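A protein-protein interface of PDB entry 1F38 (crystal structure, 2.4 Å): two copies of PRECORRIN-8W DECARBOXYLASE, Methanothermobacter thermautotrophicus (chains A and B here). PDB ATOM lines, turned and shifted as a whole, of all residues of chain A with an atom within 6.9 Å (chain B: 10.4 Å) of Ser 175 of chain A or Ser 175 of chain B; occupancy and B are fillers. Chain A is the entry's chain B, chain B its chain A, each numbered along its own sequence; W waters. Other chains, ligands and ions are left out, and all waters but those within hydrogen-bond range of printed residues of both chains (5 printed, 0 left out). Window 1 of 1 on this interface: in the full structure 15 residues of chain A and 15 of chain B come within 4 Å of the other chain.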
ATOM      1  N   ASN A 160     -27.941 -13.698 -20.097  1.00  0.00           N
ATOM      2  CA  ASN A 160     -27.896 -15.142 -20.264  1.00  0.00           C
ATOM      3  C   ASN A 160     -27.434 -15.316 -21.699  1.00  0.00           C
ATOM      4  O   ASN A 160     -28.162 -14.973 -22.629  1.00  0.00           O
ATOM      5  CB  ASN A 160     -29.264 -15.791 -20.050  1.00  0.00           C
ATOM      6  CG  ASN A 160     -29.464 -16.226 -18.631  1.00  0.00           C
ATOM      7  OD1 ASN A 160     -29.014 -17.295 -18.217  1.00  0.00           O
ATOM      8  ND2 ASN A 160     -30.135 -15.400 -17.863  1.00  0.00           N
ATOM      9  N   ILE A 161     -26.211 -15.817 -21.862  1.00  0.00           N
ATOM     10  CA  ILE A 161     -25.592 -15.998 -23.169  1.00  0.00           C
ATOM     11  C   ILE A 161     -25.359 -17.461 -23.509  1.00  0.00           C
ATOM     12  O   ILE A 161     -24.868 -18.222 -22.681  1.00  0.00           O
ATOM     13  CB  ILE A 161     -24.197 -15.341 -23.191  1.00  0.00           C
ATOM     14  CG1 ILE A 161     -24.281 -13.864 -22.813  1.00  0.00           C
ATOM     15  CG2 ILE A 161     -23.549 -15.506 -24.557  1.00  0.00           C
ATOM     16  CD1 ILE A 161     -23.078 -13.392 -21.965  1.00  0.00           C
ATOM     17  N   ALA A 162     -25.619 -17.818 -24.755  1.00  0.00           N
ATOM     18  CA  ALA A 162     -25.388 -19.155 -25.239  1.00  0.00           C
ATOM     19  C   ALA A 162     -24.635 -18.947 -26.539  1.00  0.00           C
ATOM     20  O   ALA A 162     -24.986 -18.081 -27.343  1.00  0.00           O
ATOM     21  CB  ALA A 162     -26.700 -19.876 -25.487  1.00  0.00           C
ATOM     22  N   ARG A 163     -23.561 -19.698 -26.725  1.00  0.00           N
ATOM     23  CA  ARG A 163     -22.748 -19.613 -27.934  1.00  0.00           C
ATOM     24  C   ARG A 163     -22.846 -20.970 -28.568  1.00  0.00           C
ATOM     25  O   ARG A 163     -23.002 -21.957 -27.865  1.00  0.00           O
ATOM     26  CB  ARG A 163     -21.288 -19.340 -27.599  1.00  0.00           C
ATOM     27  CG  ARG A 163     -21.053 -18.055 -26.849  1.00  0.00           C
ATOM     28  CD  ARG A 163     -19.627 -17.986 -26.380  1.00  0.00           C
ATOM     29  NE  ARG A 163     -19.395 -16.850 -25.497  1.00  0.00           N
ATOM     30  CZ  ARG A 163     -18.407 -16.788 -24.616  1.00  0.00           C
ATOM     31  NH1 ARG A 163     -17.555 -17.801 -24.488  1.00  0.00           N
ATOM     32  NH2 ARG A 163     -18.241 -15.697 -23.890  1.00  0.00           N
ATOM     33  N   MET A 173     -25.987 -25.341 -28.561  1.00  0.00           N
ATOM     34  CA  MET A 173     -25.844 -24.115 -27.811  1.00  0.00           C
ATOM     35  C   MET A 173     -25.286 -24.382 -26.440  1.00  0.00           C
ATOM     36  O   MET A 173     -25.822 -25.207 -25.698  1.00  0.00           O
ATOM     37  CB  MET A 173     -27.178 -23.371 -27.731  1.00  0.00           C
ATOM     38  CG  MET A 173     -27.847 -23.116 -29.083  1.00  0.00           C
ATOM     39  SD  MET A 173     -26.755 -22.108 -30.348  1.00  0.00           S
ATOM     40  CE  MET A 173     -26.597 -20.438 -29.318  1.00  0.00           C
ATOM     41  N   VAL A 174     -24.226 -23.664 -26.094  1.00  0.00           N
ATOM     42  CA  VAL A 174     -23.602 -23.816 -24.793  1.00  0.00           C
ATOM     43  C   VAL A 174     -23.811 -22.556 -23.964  1.00  0.00           C
ATOM     44  O   VAL A 174     -23.434 -21.459 -24.363  1.00  0.00           O
ATOM     45  CB  VAL A 174     -22.104 -24.082 -24.955  1.00  0.00           C
ATOM     46  CG1 VAL A 174     -21.465 -24.357 -23.612  1.00  0.00           C
ATOM     47  CG2 VAL A 174     -21.899 -25.229 -25.905  1.00  0.00           C
ATOM     48  N   SER A 175     -24.360 -22.718 -22.781  1.00  0.00           N
ATOM     49  CA  SER A 175     -24.659 -21.622 -21.913  1.00  0.00           C
ATOM     50  C   SER A 175     -23.508 -21.151 -21.083  1.00  0.00           C
ATOM     51  O   SER A 175     -22.588 -21.902 -20.788  1.00  0.00           O
ATOM     52  CB  SER A 175     -25.767 -22.046 -20.963  1.00  0.00           C
ATOM     53  OG  SER A 175     -27.012 -21.976 -21.634  1.00  0.00           O
ATOM     54  N   ARG A 176     -23.581 -19.898 -20.673  1.00  0.00           N
ATOM     55  CA  ARG A 176     -22.600 -19.327 -19.773  1.00  0.00           C
ATOM     56  C   ARG A 176     -23.453 -19.116 -18.560  1.00  0.00           C
ATOM     57  O   ARG A 176     -24.668 -18.964 -18.705  1.00  0.00           O
ATOM     58  CB  ARG A 176     -22.175 -17.950 -20.262  1.00  0.00           C
ATOM     59  CG  ARG A 176     -21.336 -17.963 -21.506  1.00  0.00           C
ATOM     60  CD  ARG A 176     -20.018 -18.559 -21.171  1.00  0.00           C
ATOM     61  NE  ARG A 176     -19.460 -19.359 -22.254  1.00  0.00           N
ATOM     62  CZ  ARG A 176     -18.421 -20.182 -22.111  1.00  0.00           C
ATOM     63  NH1 ARG A 176     -17.831 -20.318 -20.927  1.00  0.00           N
ATOM     64  NH2 ARG A 176     -17.918 -20.823 -23.159  1.00  0.00           N
ATOM     65  N   ASN A 177     -22.858 -19.052 -17.377  1.00  0.00           N
ATOM     66  CA  ASN A 177     -23.639 -18.787 -16.171  1.00  0.00           C
ATOM     67  C   ASN A 177     -24.152 -17.358 -16.217  1.00  0.00           C
ATOM     68  O   ASN A 177     -23.462 -16.469 -16.709  1.00  0.00           O
ATOM     69  CB  ASN A 177     -22.794 -18.966 -14.952  1.00  0.00           C
ATOM     70  CG  ASN A 177     -22.405 -20.401 -14.735  1.00  0.00           C
ATOM     71  OD1 ASN A 177     -23.009 -21.315 -15.296  1.00  0.00           O
ATOM     72  ND2 ASN A 177     -21.384 -20.617 -13.914  1.00  0.00           N
ATOM     73  N   PRO A 178     -25.358 -17.113 -15.699  1.00  0.00           N
ATOM     74  CA  PRO A 178     -25.943 -15.776 -15.701  1.00  0.00           C
ATOM     75  C   PRO A 178     -25.051 -14.773 -14.970  1.00  0.00           C
ATOM     76  O   PRO A 178     -24.516 -15.088 -13.897  1.00  0.00           O
ATOM     77  CB  PRO A 178     -27.230 -15.956 -14.899  1.00  0.00           C
ATOM     78  CG  PRO A 178     -27.507 -17.413 -14.941  1.00  0.00           C
ATOM     79  CD  PRO A 178     -26.147 -18.031 -14.866  1.00  0.00           C
ATOM     80  N   ASP B   4     -30.515 -35.719 -11.366  1.00  0.00           N
ATOM     81  CA  ASP B   4     -29.382 -35.975 -12.244  1.00  0.00           C
ATOM     82  C   ASP B   4     -28.190 -36.688 -11.619  1.00  0.00           C
ATOM     83  O   ASP B   4     -27.470 -37.425 -12.280  1.00  0.00           O
ATOM     84  CB  ASP B   4     -28.866 -34.652 -12.830  1.00  0.00           C
ATOM     85  CG  ASP B   4     -29.913 -33.885 -13.652  1.00  0.00           C
ATOM     86  OD1 ASP B   4     -31.120 -34.218 -13.663  1.00  0.00           O
ATOM     87  OD2 ASP B   4     -29.507 -32.897 -14.288  1.00  0.00           O
ATOM     88  N   ALA B  18     -31.588 -32.979 -18.242  1.00  0.00           N
ATOM     89  CA  ALA B  18     -31.826 -32.245 -17.008  1.00  0.00           C
ATOM     90  C   ALA B  18     -33.165 -32.636 -16.391  1.00  0.00           C
ATOM     91  O   ALA B  18     -34.173 -32.805 -17.087  1.00  0.00           O
ATOM     92  CB  ALA B  18     -31.784 -30.730 -17.250  1.00  0.00           C
ATOM     93  N   GLU B  20     -35.292 -30.891 -14.923  1.00  0.00           N
ATOM     94  CA  GLU B  20     -36.335 -29.921 -15.229  1.00  0.00           C
ATOM     95  C   GLU B  20     -36.923 -30.164 -16.613  1.00  0.00           C
ATOM     96  O   GLU B  20     -38.094 -29.884 -16.859  1.00  0.00           O
ATOM     97  CB  GLU B  20     -35.810 -28.507 -15.156  1.00  0.00           C
ATOM     98  CG  GLU B  20     -35.424 -28.053 -13.789  1.00  0.00           C
ATOM     99  CD  GLU B  20     -34.040 -28.514 -13.377  1.00  0.00           C
ATOM    100  OE1 GLU B  20     -33.361 -29.206 -14.158  1.00  0.00           O
ATOM    101  OE2 GLU B  20     -33.609 -28.183 -12.254  1.00  0.00           O
ATOM    102  N   ILE B 135     -30.969 -30.336 -29.028  1.00  0.00           N
ATOM    103  CA  ILE B 135     -29.746 -29.734 -28.516  1.00  0.00           C
ATOM    104  C   ILE B 135     -29.099 -28.909 -29.599  1.00  0.00           C
ATOM    105  O   ILE B 135     -28.516 -27.886 -29.341  1.00  0.00           O
ATOM    106  CB  ILE B 135     -28.795 -30.846 -28.096  1.00  0.00           C
ATOM    107  CG1 ILE B 135     -29.339 -31.479 -26.833  1.00  0.00           C
ATOM    108  CG2 ILE B 135     -27.407 -30.337 -27.866  1.00  0.00           C
ATOM    109  CD1 ILE B 135     -29.888 -30.444 -25.869  1.00  0.00           C
ATOM    110  N   LYS B 140     -33.780 -28.379 -34.110  1.00  0.00           N
ATOM    111  CA  LYS B 140     -34.933 -27.534 -33.808  1.00  0.00           C
ATOM    112  C   LYS B 140     -35.677 -27.214 -35.112  1.00  0.00           C
ATOM    113  O   LYS B 140     -36.902 -27.319 -35.184  1.00  0.00           O
ATOM    114  CB  LYS B 140     -34.489 -26.238 -33.108  1.00  0.00           C
ATOM    115  CG  LYS B 140     -33.814 -26.481 -31.750  1.00  0.00           C
ATOM    116  CD  LYS B 140     -33.263 -25.212 -31.105  1.00  0.00           C
ATOM    117  CE  LYS B 140     -32.477 -25.569 -29.859  1.00  0.00           C
ATOM    118  NZ  LYS B 140     -31.679 -24.406 -29.389  1.00  0.00           N
ATOM    119  N   GLU B 158     -38.310 -23.577 -25.382  1.00  0.00           N
ATOM    120  CA  GLU B 158     -36.907 -23.701 -25.038  1.00  0.00           C
ATOM    121  C   GLU B 158     -36.772 -23.437 -23.565  1.00  0.00           C
ATOM    122  O   GLU B 158     -37.318 -22.455 -23.030  1.00  0.00           O
ATOM    123  CB  GLU B 158     -36.049 -22.682 -25.752  1.00  0.00           C
ATOM    124  CG  GLU B 158     -35.800 -22.971 -27.181  1.00  0.00           C
ATOM    125  CD  GLU B 158     -34.335 -22.813 -27.552  1.00  0.00           C
ATOM    126  OE1 GLU B 158     -33.461 -22.947 -26.647  1.00  0.00           O
ATOM    127  OE2 GLU B 158     -34.075 -22.580 -28.766  1.00  0.00           O
ATOM    128  N   LEU B 159     -35.914 -24.225 -22.947  1.00  0.00           N
ATOM    129  CA  LEU B 159     -35.689 -24.072 -21.538  1.00  0.00           C
ATOM    130  C   LEU B 159     -34.282 -23.701 -21.224  1.00  0.00           C
ATOM    131  O   LEU B 159     -33.367 -24.368 -21.674  1.00  0.00           O
ATOM    132  CB  LEU B 159     -35.985 -25.379 -20.815  1.00  0.00           C
ATOM    133  CG  LEU B 159     -37.453 -25.764 -20.717  1.00  0.00           C
ATOM    134  CD1 LEU B 159     -37.589 -26.768 -19.626  1.00  0.00           C
ATOM    135  CD2 LEU B 159     -38.245 -24.536 -20.356  1.00  0.00           C
ATOM    136  N   ASN B 160     -34.118 -22.633 -20.460  1.00  0.00           N
ATOM    137  CA  ASN B 160     -32.816 -22.204 -20.008  1.00  0.00           C
ATOM    138  C   ASN B 160     -32.943 -22.301 -18.511  1.00  0.00           C
ATOM    139  O   ASN B 160     -33.684 -21.520 -17.908  1.00  0.00           O
ATOM    140  CB  ASN B 160     -32.551 -20.764 -20.411  1.00  0.00           C
ATOM    141  CG  ASN B 160     -31.828 -20.676 -21.709  1.00  0.00           C
ATOM    142  OD1 ASN B 160     -30.608 -20.850 -21.747  1.00  0.00           O
ATOM    143  ND2 ASN B 160     -32.570 -20.457 -22.801  1.00  0.00           N
ATOM    144  N   ILE B 161     -32.188 -23.231 -17.918  1.00  0.00           N
ATOM    145  CA  ILE B 161     -32.201 -23.492 -16.471  1.00  0.00           C
ATOM    146  C   ILE B 161     -30.917 -23.127 -15.745  1.00  0.00           C
ATOM    147  O   ILE B 161     -29.846 -23.480 -16.196  1.00  0.00           O
ATOM    148  CB  ILE B 161     -32.402 -24.987 -16.223  1.00  0.00           C
ATOM    149  CG1 ILE B 161     -33.690 -25.456 -16.880  1.00  0.00           C
ATOM    150  CG2 ILE B 161     -32.474 -25.282 -14.724  1.00  0.00           C
ATOM    151  CD1 ILE B 161     -33.557 -26.905 -17.374  1.00  0.00           C
ATOM    152  N   ALA B 162     -31.026 -22.519 -14.575  1.00  0.00           N
ATOM    153  CA  ALA B 162     -29.846 -22.174 -13.782  1.00  0.00           C
ATOM    154  C   ALA B 162     -30.131 -22.693 -12.402  1.00  0.00           C
ATOM    155  O   ALA B 162     -31.216 -22.456 -11.873  1.00  0.00           O
ATOM    156  CB  ALA B 162     -29.655 -20.703 -13.717  1.00  0.00           C
ATOM    157  N   ARG B 163     -29.186 -23.399 -11.806  1.00  0.00           N
ATOM    158  CA  ARG B 163     -29.402 -23.963 -10.484  1.00  0.00           C
ATOM    159  C   ARG B 163     -28.341 -23.309  -9.650  1.00  0.00           C
ATOM    160  O   ARG B 163     -27.299 -22.939 -10.183  1.00  0.00           O
ATOM    161  CB  ARG B 163     -29.155 -25.466 -10.505  1.00  0.00           C
ATOM    162  CG  ARG B 163     -30.008 -26.250 -11.477  1.00  0.00           C
ATOM    163  CD  ARG B 163     -29.593 -27.690 -11.455  1.00  0.00           C
ATOM    164  NE  ARG B 163     -30.353 -28.497 -12.399  1.00  0.00           N
ATOM    165  CZ  ARG B 163     -29.904 -29.602 -12.987  1.00  0.00           C
ATOM    166  NH1 ARG B 163     -28.683 -30.054 -12.727  1.00  0.00           N
ATOM    167  NH2 ARG B 163     -30.670 -30.248 -13.863  1.00  0.00           N
ATOM    168  N   GLY B 164     -28.589 -23.126  -8.360  1.00  0.00           N
ATOM    169  CA  GLY B 164     -27.593 -22.481  -7.518  1.00  0.00           C
ATOM    170  C   GLY B 164     -26.588 -23.438  -6.943  1.00  0.00           C
ATOM    171  O   GLY B 164     -26.962 -24.532  -6.547  1.00  0.00           O
ATOM    172  N   ARG B 165     -25.314 -23.071  -6.965  1.00  0.00           N
ATOM    173  CA  ARG B 165     -24.267 -23.912  -6.382  1.00  0.00           C
ATOM    174  C   ARG B 165     -23.780 -23.227  -5.111  1.00  0.00           C
ATOM    175  O   ARG B 165     -23.374 -22.072  -5.121  1.00  0.00           O
ATOM    176  CB  ARG B 165     -23.083 -24.122  -7.328  1.00  0.00           C
ATOM    177  CG  ARG B 165     -22.000 -25.017  -6.719  1.00  0.00           C
ATOM    178  CD  ARG B 165     -20.787 -25.206  -7.623  1.00  0.00           C
ATOM    179  NE  ARG B 165     -21.123 -25.924  -8.852  1.00  0.00           N
ATOM    180  CZ  ARG B 165     -20.538 -25.695 -10.021  1.00  0.00           C
ATOM    181  NH1 ARG B 165     -19.585 -24.764 -10.117  1.00  0.00           N
ATOM    182  NH2 ARG B 165     -20.917 -26.382 -11.093  1.00  0.00           N
ATOM    183  N   MET B 172     -23.815 -19.257  -6.301  1.00  0.00           N
ATOM    184  CA  MET B 172     -23.693 -18.855  -7.685  1.00  0.00           C
ATOM    185  C   MET B 172     -24.635 -19.640  -8.606  1.00  0.00           C
ATOM    186  O   MET B 172     -24.884 -20.838  -8.407  1.00  0.00           O
ATOM    187  CB  MET B 172     -22.263 -19.000  -8.156  1.00  0.00           C
ATOM    188  CG  MET B 172     -21.890 -20.380  -8.543  1.00  0.00           C
ATOM    189  SD  MET B 172     -20.435 -20.107  -9.673  1.00  0.00           S
ATOM    190  CE  MET B 172     -19.369 -21.653  -9.274  1.00  0.00           C
ATOM    191  N   MET B 173     -25.133 -18.972  -9.637  1.00  0.00           N
ATOM    192  CA  MET B 173     -26.030 -19.644 -10.552  1.00  0.00           C
ATOM    193  C   MET B 173     -25.262 -20.325 -11.641  1.00  0.00           C
ATOM    194  O   MET B 173     -24.446 -19.707 -12.288  1.00  0.00           O
ATOM    195  CB  MET B 173     -27.056 -18.672 -11.130  1.00  0.00           C
ATOM    196  CG  MET B 173     -27.835 -17.857 -10.068  1.00  0.00           C
ATOM    197  SD  MET B 173     -28.866 -18.861  -8.787  1.00  0.00           S
ATOM    198  CE  MET B 173     -30.016 -19.800 -10.053  1.00  0.00           C
ATOM    199  N   VAL B 174     -25.543 -21.607 -11.831  1.00  0.00           N
ATOM    200  CA  VAL B 174     -24.870 -22.395 -12.847  1.00  0.00           C
ATOM    201  C   VAL B 174     -25.867 -22.799 -13.932  1.00  0.00           C
ATOM    202  O   VAL B 174     -26.854 -23.468 -13.667  1.00  0.00           O
ATOM    203  CB  VAL B 174     -24.240 -23.662 -12.216  1.00  0.00           C
ATOM    204  CG1 VAL B 174     -23.418 -24.411 -13.245  1.00  0.00           C
ATOM    205  CG2 VAL B 174     -23.369 -23.272 -11.051  1.00  0.00           C
ATOM    206  N   SER B 175     -25.565 -22.443 -15.161  1.00  0.00           N
ATOM    207  CA  SER B 175     -26.410 -22.735 -16.290  1.00  0.00           C
ATOM    208  C   SER B 175     -26.323 -24.101 -16.869  1.00  0.00           C
ATOM    209  O   SER B 175     -25.301 -24.782 -16.771  1.00  0.00           O
ATOM    210  CB  SER B 175     -26.071 -21.794 -17.411  1.00  0.00           C
ATOM    211  OG  SER B 175     -26.561 -20.507 -17.059  1.00  0.00           O
ATOM    212  N   ARG B 176     -27.413 -24.497 -17.497  1.00  0.00           N
ATOM    213  CA  ARG B 176     -27.456 -25.762 -18.207  1.00  0.00           C
ATOM    214  C   ARG B 176     -27.549 -25.275 -19.642  1.00  0.00           C
ATOM    215  O   ARG B 176     -28.019 -24.171 -19.893  1.00  0.00           O
ATOM    216  CB  ARG B 176     -28.733 -26.521 -17.888  1.00  0.00           C
ATOM    217  CG  ARG B 176     -28.793 -27.040 -16.491  1.00  0.00           C
ATOM    218  CD  ARG B 176     -27.746 -28.078 -16.366  1.00  0.00           C
ATOM    219  NE  ARG B 176     -27.187 -28.159 -15.027  1.00  0.00           N
ATOM    220  CZ  ARG B 176     -26.149 -28.917 -14.709  1.00  0.00           C
ATOM    221  NH1 ARG B 176     -25.567 -29.650 -15.646  1.00  0.00           N
ATOM    222  NH2 ARG B 176     -25.712 -28.956 -13.454  1.00  0.00           N
ATOM    223  N   ASN B 177     -27.093 -26.070 -20.588  1.00  0.00           N
ATOM    224  CA  ASN B 177     -27.209 -25.666 -21.978  1.00  0.00           C
ATOM    225  C   ASN B 177     -28.678 -25.651 -22.357  1.00  0.00           C
ATOM    226  O   ASN B 177     -29.456 -26.492 -21.910  1.00  0.00           O
ATOM    227  CB  ASN B 177     -26.453 -26.621 -22.881  1.00  0.00           C
ATOM    228  CG  ASN B 177     -24.962 -26.556 -22.671  1.00  0.00           C
ATOM    229  OD1 ASN B 177     -24.435 -25.600 -22.116  1.00  0.00           O
ATOM    230  ND2 ASN B 177     -24.277 -27.590 -23.104  1.00  0.00           N
ATOM    231  N   PRO B 178     -29.078 -24.741 -23.225  1.00  0.00           N
ATOM    232  CA  PRO B 178     -30.482 -24.653 -23.643  1.00  0.00           C
ATOM    233  C   PRO B 178     -30.987 -25.930 -24.276  1.00  0.00           C
ATOM    234  O   PRO B 178     -30.291 -26.554 -25.059  1.00  0.00           O
ATOM    235  CB  PRO B 178     -30.447 -23.552 -24.709  1.00  0.00           C
ATOM    236  CG  PRO B 178     -29.187 -22.772 -24.397  1.00  0.00           C
ATOM    237  CD  PRO B 178     -28.229 -23.841 -24.009  1.00  0.00           C
ATOM    238  N   VAL B 179     -32.222 -26.283 -23.985  1.00  0.00           N
ATOM    239  CA  VAL B 179     -32.819 -27.486 -24.557  1.00  0.00           C
ATOM    240  C   VAL B 179     -34.182 -27.091 -25.118  1.00  0.00           C
ATOM    241  O   VAL B 179     -34.920 -26.311 -24.484  1.00  0.00           O
ATOM    242  CB  VAL B 179     -33.067 -28.552 -23.493  1.00  0.00           C
ATOM    243  CG1 VAL B 179     -33.656 -29.789 -24.145  1.00  0.00           C
ATOM    244  CG2 VAL B 179     -31.764 -28.904 -22.797  1.00  0.00           C
HETATM  245  O   HOH W   1     -27.267 -27.817 -25.600  1.00  0.00           O
HETATM  246  O   HOH W   2     -22.552 -16.822 -12.583  1.00  0.00           O
HETATM  247  O   HOH W   3     -22.693 -24.975 -19.795  1.00  0.00           O
HETATM  248  O   HOH W   4     -28.389 -19.125 -22.184  1.00  0.00           O
HETATM  249  O   HOH W   5     -29.466 -19.874 -17.246  1.00  0.00           O
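Asn 160 of chain A touches none of the printed residues of chain B. Ile 161 of chain A touches none of the printed residues of chain B. Of the printed residues of chain B, Ala 162 of chain A touches Pro 178. Of the printed residues of chain B, Met 173 of chain A touches Ile 135, Asn 177 and Pro 178. Of chain B, only Ser 175 (2.9 Å) comes within 4 Å of Arg 176 of chain A. Of the printed residues of chain A, Val 174 of chain B touches Asn 177 (3.3 Å). Of chain A, only Ser 175, Arg 176, Asn 177 and Pro 178 come within 4 Å of Ser 175 of chain B. Printed residues of chain A within 4 Å of Asn 177 of chain B: Met 173, Val 174 and Ser 175. Printed residues of chain A within 4 Å of Pro 178 of chain B: Ala 162, Met 173 and Ser 175. The nearest residue of chain B that does not touch Ser 175 of chain A is Ile 161 of chain B (6.3 Å).
The side-chain hydroxyl (OG) of Ser 175 of chain B is in hydrogen-bond range of the backbone carbonyl oxygen (O) of Arg 176 of chain A (2.9 Å). The backbone NH (N) of Ser 175 of chain B sits at hydrogen-bond distance from the side-chain amide oxygen (OD1) of Asn 177 of chain A (2.8 Å). O of Arg 176 of chain B lies within hydrogen-bond range of OG of Ser 175 of chain A (3.0 Å). The side-chain amide oxygen (OD1) of Asn 177 of chain B is in hydrogen-bond range of the backbone NH (N) of Ser 175 of chain A, at 3.0 Å.
Ala 162 of chain A touches Pro 178 of chain B, but with the chains exchanged Pro 178 of chain A does not touch Ala 162 of chain B (4.1 Å). Met 173 of chain A touches Asn 177 of chain B, and with the chains exchanged Asn 177 of chain A touches Met 173 of chain B. Ser 175 of chain A touches Asn 160 of chain B, but with the chains exchanged Asn 160 of chain A does not touch Ser 175 of chain B (4.2 Å). Ser 175 of chain A touches its own counterpart, Ser 175 of chain B. Positions printed for both chains: 160, 161, 162, 163, 173, 174, 175, 176, 177 and 178.
Water W5 bridges OD1 of Asn 160 of chain A and OG of Ser 175 of chain B. Water W4 lies within hydrogen-bond range of the side-chain amide oxygen of Asn 160 of chain B and the side-chain hydroxyl of Ser 175 of chain A. Water W2 lies within hydrogen-bond range of O of Pro 178 of chain A and O of Met 173 of chain B. Water W3 bridges the side-chain amide oxygen of Asn 177 of chain B (3.0 Å) and the backbone carbonyl oxygen of Ser 175 of chain A (3.2 Å). Water W1 bridges O of Met 173 of chain A (3.0 Å) and O of Pro 178 of chain B (3.3 Å).
Of the 21 printed residues of chain B, 8 touch a printed residue of chain A. Hydrophobic or aromatic side chains of chain B that line the printed part of chain A: Met 173, Val 174 and Pro 178. Hydrophobic or aromatic side chains of chain A within 4 Å of the printed part of chain B: Ala 162, Met 173, Val 174 and Pro 178. Among the printed residues, 16 pairs touch across the chains. Among the printed residues, no Asp or Glu carboxylate lies within 4 Å of a Lys or Arg side-chain nitrogen of the other chain.
The backbone NH (N) of Arg 176 of chain B lies within hydrogen-bond range of the backbone carbonyl oxygen (O) of Ile 161 of chain B. The backbone NH (N) of Val 174 of chain B lies within hydrogen-bond range of the backbone carbonyl oxygen (O) of Arg 163 of chain B (2.8 Å). O of Ile 161 of chain A lies within hydrogen-bond range of N of Arg 176 of chain A, at 2.9 Å. The backbone carbonyl oxygen (O) of Arg 163 of chain A sits at hydrogen-bond distance from the backbone NH (N) of Val 174 of chain A (2.7 Å).
Ala 162 of chain A touches Pro 178 of chain B (CB to CG, 3.97 Å). Met 173 of chain A touches Ile 135 of chain B (N to O, 3.7 Å). Met 173 of chain A touches Asn 177 of chain B. Met 173 of chain A touches Pro 178 of chain B. Asn 177 of chain B touches Val 174 of chain A (OD1 to CA, 3.3 Å). Asn 160 of chain B touches Ser 175 of chain A. CB of Ser 175 of chain B touches CB of Ser 175 of chain A, 3.6 Å away. Pro 178 of chain B touches Ser 175 of chain A (CD to OG, 3.3 Å). CA of Val 174 of chain B touches OD1 of Asn 177 of chain A (3.3 Å). OG of Ser 175 of chain B touches CD of Pro 178 of chain A, at 3.3 Å.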
